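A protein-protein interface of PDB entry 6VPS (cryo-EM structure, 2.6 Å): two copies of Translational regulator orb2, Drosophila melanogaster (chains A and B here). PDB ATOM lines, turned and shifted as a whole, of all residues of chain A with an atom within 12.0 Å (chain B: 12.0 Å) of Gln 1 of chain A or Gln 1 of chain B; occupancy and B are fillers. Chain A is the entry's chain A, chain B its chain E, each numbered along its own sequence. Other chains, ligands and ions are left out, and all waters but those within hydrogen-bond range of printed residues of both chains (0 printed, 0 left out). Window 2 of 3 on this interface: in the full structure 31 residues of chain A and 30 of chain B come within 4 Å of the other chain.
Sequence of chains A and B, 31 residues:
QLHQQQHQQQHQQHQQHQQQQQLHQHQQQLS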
ATOM      1  N   GLN A   1     -15.865   1.924   3.433  1.00  0.00           N
ATOM      2  CA  GLN A   1     -14.569   2.259   4.118  1.00  0.00           C
ATOM      3  C   GLN A   1     -14.138   3.675   3.708  1.00  0.00           C
ATOM      4  O   GLN A   1     -13.627   3.883   2.605  1.00  0.00           O
ATOM      5  CB  GLN A   1     -13.514   1.178   3.821  1.00  0.00           C
ATOM      6  CG  GLN A   1     -12.427   1.057   4.890  1.00  0.00           C
ATOM      7  CD  GLN A   1     -11.209   1.911   4.610  1.00  0.00           C
ATOM      8  OE1 GLN A   1     -10.484   1.696   3.640  1.00  0.00           O
ATOM      9  NE2 GLN A   1     -10.933   2.842   5.510  1.00  0.00           N
ATOM     10  N   LEU A   2     -14.374   4.640   4.614  1.00  0.00           N
ATOM     11  CA  LEU A   2     -14.169   6.059   4.340  1.00  0.00           C
ATOM     12  C   LEU A   2     -13.042   6.610   5.219  1.00  0.00           C
ATOM     13  O   LEU A   2     -13.043   6.428   6.438  1.00  0.00           O
ATOM     14  CB  LEU A   2     -15.501   6.804   4.553  1.00  0.00           C
ATOM     15  CG  LEU A   2     -15.445   8.342   4.626  1.00  0.00           C
ATOM     16  CD1 LEU A   2     -14.953   8.958   3.317  1.00  0.00           C
ATOM     17  CD2 LEU A   2     -16.805   8.907   4.990  1.00  0.00           C
ATOM     18  N   HIS A   3     -12.113   7.329   4.568  1.00  0.00           N
ATOM     19  CA  HIS A   3     -10.961   7.931   5.212  1.00  0.00           C
ATOM     20  C   HIS A   3     -10.950   9.434   4.920  1.00  0.00           C
ATOM     21  O   HIS A   3     -10.788   9.845   3.765  1.00  0.00           O
ATOM     22  CB  HIS A   3      -9.680   7.232   4.744  1.00  0.00           C
ATOM     23  CG  HIS A   3      -8.511   7.461   5.635  1.00  0.00           C
ATOM     24  ND1 HIS A   3      -7.978   6.457   6.424  1.00  0.00           N
ATOM     25  CD2 HIS A   3      -7.784   8.572   5.892  1.00  0.00           C
ATOM     26  CE1 HIS A   3      -6.967   6.937   7.115  1.00  0.00           C
ATOM     27  NE2 HIS A   3      -6.830   8.233   6.811  1.00  0.00           N
ATOM     28  N   GLN A   4     -11.185  10.235   5.967  1.00  0.00           N
ATOM     29  CA  GLN A   4     -11.179  11.692   5.873  1.00  0.00           C
ATOM     30  C   GLN A   4     -10.005  12.239   6.698  1.00  0.00           C
ATOM     31  O   GLN A   4      -9.953  12.043   7.921  1.00  0.00           O
ATOM     32  CB  GLN A   4     -12.485  12.277   6.435  1.00  0.00           C
ATOM     33  CG  GLN A   4     -13.742  11.915   5.659  1.00  0.00           C
ATOM     34  CD  GLN A   4     -14.975  12.616   6.212  1.00  0.00           C
ATOM     35  OE1 GLN A   4     -15.231  12.630   7.434  1.00  0.00           O
ATOM     36  NE2 GLN A   4     -15.776  13.187   5.313  1.00  0.00           N
ATOM     37  N   GLN A   5      -9.068  12.927   6.032  1.00  0.00           N
ATOM     38  CA  GLN A   5      -8.008  13.605   6.757  1.00  0.00           C
ATOM     39  C   GLN A   5      -7.931  15.055   6.369  1.00  0.00           C
ATOM     40  O   GLN A   5      -8.082  15.404   5.197  1.00  0.00           O
ATOM     41  CB  GLN A   5      -6.674  12.865   6.735  1.00  0.00           C
ATOM     42  CG  GLN A   5      -6.215  12.399   5.380  1.00  0.00           C
ATOM     43  CD  GLN A   5      -4.926  11.621   5.493  1.00  0.00           C
ATOM     44  OE1 GLN A   5      -4.888  10.518   6.042  1.00  0.00           O
ATOM     45  NE2 GLN A   5      -3.849  12.194   4.976  1.00  0.00           N
ATOM     46  N   LEU A  30     -17.943  15.756   8.336  1.00  0.00           N
ATOM     47  CA  LEU A  30     -19.258  15.137   8.525  1.00  0.00           C
ATOM     48  C   LEU A  30     -19.299  13.767   7.844  1.00  0.00           C
ATOM     49  O   LEU A  30     -18.537  13.511   6.905  1.00  0.00           O
ATOM     50  CB  LEU A  30     -20.338  16.058   7.958  1.00  0.00           C
ATOM     51  CG  LEU A  30     -20.636  17.310   8.778  1.00  0.00           C
ATOM     52  CD1 LEU A  30     -19.988  18.528   8.149  1.00  0.00           C
ATOM     53  CD2 LEU A  30     -22.135  17.523   8.891  1.00  0.00           C
ATOM     54  N   SER A  31     -20.211  12.896   8.339  1.00  0.00           N
ATOM     55  CA  SER A  31     -20.498  11.586   7.750  1.00  0.00           C
ATOM     56  C   SER A  31     -22.011  11.311   7.797  1.00  0.00           C
ATOM     57  O   SER A  31     -22.770  12.165   7.282  1.00  0.00           O
ATOM     58  CB  SER A  31     -19.730  10.499   8.442  1.00  0.00           C
ATOM     59  OG  SER A  31     -18.343  10.657   8.233  1.00  0.00           O
ATOM     60  N   GLN B   1     -16.753   1.216   8.034  1.00  0.00           N
ATOM     61  CA  GLN B   1     -15.466   1.445   8.775  1.00  0.00           C
ATOM     62  C   GLN B   1     -14.939   2.849   8.440  1.00  0.00           C
ATOM     63  O   GLN B   1     -14.219   3.039   7.454  1.00  0.00           O
ATOM     64  CB  GLN B   1     -14.467   0.313   8.478  1.00  0.00           C
ATOM     65  CG  GLN B   1     -13.474   0.043   9.611  1.00  0.00           C
ATOM     66  CD  GLN B   1     -12.221   0.888   9.538  1.00  0.00           C
ATOM     67  OE1 GLN B   1     -11.466   0.834   8.567  1.00  0.00           O
ATOM     68  NE2 GLN B   1     -11.949   1.619  10.606  1.00  0.00           N
ATOM     69  N   LEU B   2     -15.326   3.824   9.280  1.00  0.00           N
ATOM     70  CA  LEU B   2     -15.049   5.239   9.063  1.00  0.00           C
ATOM     71  C   LEU B   2     -13.836   5.672   9.896  1.00  0.00           C
ATOM     72  O   LEU B   2     -13.715   5.313  11.071  1.00  0.00           O
ATOM     73  CB  LEU B   2     -16.316   6.044   9.421  1.00  0.00           C
ATOM     74  CG  LEU B   2     -16.139   7.551   9.677  1.00  0.00           C
ATOM     75  CD1 LEU B   2     -15.854   8.304   8.389  1.00  0.00           C
ATOM     76  CD2 LEU B   2     -17.363   8.131  10.368  1.00  0.00           C
ATOM     77  N   HIS B   3     -12.967   6.481   9.266  1.00  0.00           N
ATOM     78  CA  HIS B   3     -11.774   7.023   9.890  1.00  0.00           C
ATOM     79  C   HIS B   3     -11.699   8.523   9.609  1.00  0.00           C
ATOM     80  O   HIS B   3     -11.599   8.938   8.452  1.00  0.00           O
ATOM     81  CB  HIS B   3     -10.535   6.275   9.383  1.00  0.00           C
ATOM     82  CG  HIS B   3      -9.331   6.466  10.234  1.00  0.00           C
ATOM     83  ND1 HIS B   3      -8.815   5.448  11.018  1.00  0.00           N
ATOM     84  CD2 HIS B   3      -8.559   7.551  10.466  1.00  0.00           C
ATOM     85  CE1 HIS B   3      -7.768   5.896  11.679  1.00  0.00           C
ATOM     86  NE2 HIS B   3      -7.592   7.183  11.358  1.00  0.00           N
ATOM     87  N   GLN B   4     -11.781   9.323  10.676  1.00  0.00           N
ATOM     88  CA  GLN B   4     -11.735  10.778  10.574  1.00  0.00           C
ATOM     89  C   GLN B   4     -10.541  11.294  11.377  1.00  0.00           C
ATOM     90  O   GLN B   4     -10.467  11.078  12.587  1.00  0.00           O
ATOM     91  CB  GLN B   4     -13.018  11.400  11.146  1.00  0.00           C
ATOM     92  CG  GLN B   4     -14.296  10.995  10.437  1.00  0.00           C
ATOM     93  CD  GLN B   4     -15.502  11.771  10.946  1.00  0.00           C
ATOM     94  OE1 GLN B   4     -15.742  11.882  12.161  1.00  0.00           O
ATOM     95  NE2 GLN B   4     -16.295  12.297  10.015  1.00  0.00           N
ATOM     96  N   GLN B   5      -9.601  11.963  10.699  1.00  0.00           N
ATOM     97  CA  GLN B   5      -8.513  12.626  11.403  1.00  0.00           C
ATOM     98  C   GLN B   5      -8.434  14.077  11.029  1.00  0.00           C
ATOM     99  O   GLN B   5      -8.743  14.458   9.887  1.00  0.00           O
ATOM    100  CB  GLN B   5      -7.187  11.879  11.355  1.00  0.00           C
ATOM    101  CG  GLN B   5      -6.833  11.290  10.014  1.00  0.00           C
ATOM    102  CD  GLN B   5      -5.565  10.476  10.099  1.00  0.00           C
ATOM    103  OE1 GLN B   5      -5.517   9.428  10.745  1.00  0.00           O
ATOM    104  NE2 GLN B   5      -4.518  10.954   9.440  1.00  0.00           N
ATOM    105  N   LEU B  30     -18.447  14.932  13.024  1.00  0.00           N
ATOM    106  CA  LEU B  30     -19.780  14.357  13.194  1.00  0.00           C
ATOM    107  C   LEU B  30     -19.860  12.985  12.523  1.00  0.00           C
ATOM    108  O   LEU B  30     -19.065  12.676  11.629  1.00  0.00           O
ATOM    109  CB  LEU B  30     -20.817  15.314  12.613  1.00  0.00           C
ATOM    110  CG  LEU B  30     -21.161  16.517  13.486  1.00  0.00           C
ATOM    111  CD1 LEU B  30     -20.396  17.746  13.034  1.00  0.00           C
ATOM    112  CD2 LEU B  30     -22.652  16.791  13.442  1.00  0.00           C
ATOM    113  N   SER B  31     -20.832  12.165  12.990  1.00  0.00           N
ATOM    114  CA  SER B  31     -21.168  10.868  12.401  1.00  0.00           C
ATOM    115  C   SER B  31     -22.688  10.635  12.477  1.00  0.00           C
ATOM    116  O   SER B  31     -23.437  11.551  12.061  1.00  0.00           O
ATOM    117  CB  SER B  31     -20.419   9.754  13.074  1.00  0.00           C
ATOM    118  OG  SER B  31     -19.029   9.870  12.836  1.00  0.00           O
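Leu 2 of chain A touches Gln 1 of chain B, but with the chains exchanged Gln 1 of chain A does not touch Leu 2 of chain B (5.4 Å).
His 3 of chain A touches its own counterpart, His 3 of chain B.
Leu 30 of chain A touches its own counterpart, Leu 30 of chain B.
Ser 31 of chain A touches Leu 2 of chain B, but with the chains exchanged Leu 2 of chain A does not touch Ser 31 of chain B (8.2 Å).
7 positions are printed for both chains.
Of the 14 pairs that touch across the chains among the printed residues, 6 have their exchanged pair printed and touching as well.
N of Gln 4 of chain A sits at hydrogen-bond distance from O of His 3 of chain B.
O of Gln 1 of chain B sits at hydrogen-bond distance from N of Leu 2 of chain A (3.3 Å).
O of Gln 4 of chain A lies within hydrogen-bond range of N of Gln 5 of chain B.
The backbone carbonyl oxygen (O) of Leu 30 of chain B is in hydrogen-bond range of the backbone NH (N) of Ser 31 of chain A (3.5 Å).
The side-chain amide nitrogen (NE2) of Gln 5 of chain B lies within hydrogen-bond range of the side-chain amide oxygen (OE1) of Gln 5 of chain A (3.4 Å).
The backbone NH (N) of His 3 of chain B sits at hydrogen-bond distance from the backbone carbonyl oxygen (O) of Leu 2 of chain A (2.8 Å).
The side-chain hydroxyl (OG) of Ser 31 of chain A sits at hydrogen-bond distance from the side-chain amide nitrogen (NE2) of Gln 4 of chain B.
OE1 of Gln 4 of chain A sits at hydrogen-bond distance from NE2 of Gln 4 of chain B, at 2.8 Å.
The side-chain amide oxygen (OE1) of Gln 5 of chain A lies within hydrogen-bond range of a ring nitrogen (NE2) of His 3 of chain A, 3.1 Å away.
NE2 of Gln 4 of chain B sits at hydrogen-bond distance from O of Leu 30 of chain B (3.2 Å).
The side-chain amide nitrogen of Gln 4 of chain A sits at hydrogen-bond distance from the backbone carbonyl oxygen of Leu 30 of chain A, 3.2 Å away.
A ring nitrogen (NE2) of His 3 of chain B sits at hydrogen-bond distance from the side-chain amide oxygen of Gln 5 of chain B, at 3.1 Å.
Among the printed residues, pairs that only touch across the chains: Ser 31 of chain A with Leu 2 of chain B (3.4 Å), Gln 1 of chain A with Gln 1 of chain B (3.4 Å), His 3 of chain A with His 3 of chain B (3.5 Å), Leu 2 of chain A with Leu 2 of chain B (3.5 Å), Leu 30 of chain A with Leu 30 of chain B (3.9 Å) and Leu 30 of chain A with Gln 4 of chain B (3.99 Å).
Of chain B, only Gln 1 (3.4 Å) comes within 4 Å of Gln 1 of chain A.
His 3 of chain A touches just one residue of chain B: His 3.
Leu 2 of chain B touches just these residues of chain A: Leu 2 and Ser 31.
His 3 of chain B touches just these residues of chain A: Leu 2 (2.8 Å), His 3 (3.5 Å) and Gln 4 (2.8 Å).
Of the printed residues of chain B, Gln 5 of chain A touches Gln 5.
Printed residues of chain B within 4 Å of Ser 31 of chain A: Leu 2, Gln 4 and Leu 30.
Printed residues of chain A within 4 Å of Gln 5 of chain B: Gln 4 and Gln 5.
Of the printed residues of chain B, Leu 30 of chain A touches Gln 4 and Leu 30.
Printed residues of chain A within 4 Å of Leu 30 of chain B: Leu 30 (3.9 Å) and Ser 31 (3.5 Å).
The nearest residue of chain B that does not touch Gln 1 of chain A is His 3 of chain B (5.2 Å).
Of the 7 printed residues of chain B, 6 touch a printed residue of chain A.
Along chain B the printed residues that touch a printed residue of chain A span positions 1 to 30.
Of the 7 printed residues of chain A, 7 touch a printed residue of chain B.
Among the printed residues, no Asp or Glu carboxylate lies within 4 Å of a Lys or Arg side-chain nitrogen of the other chain.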
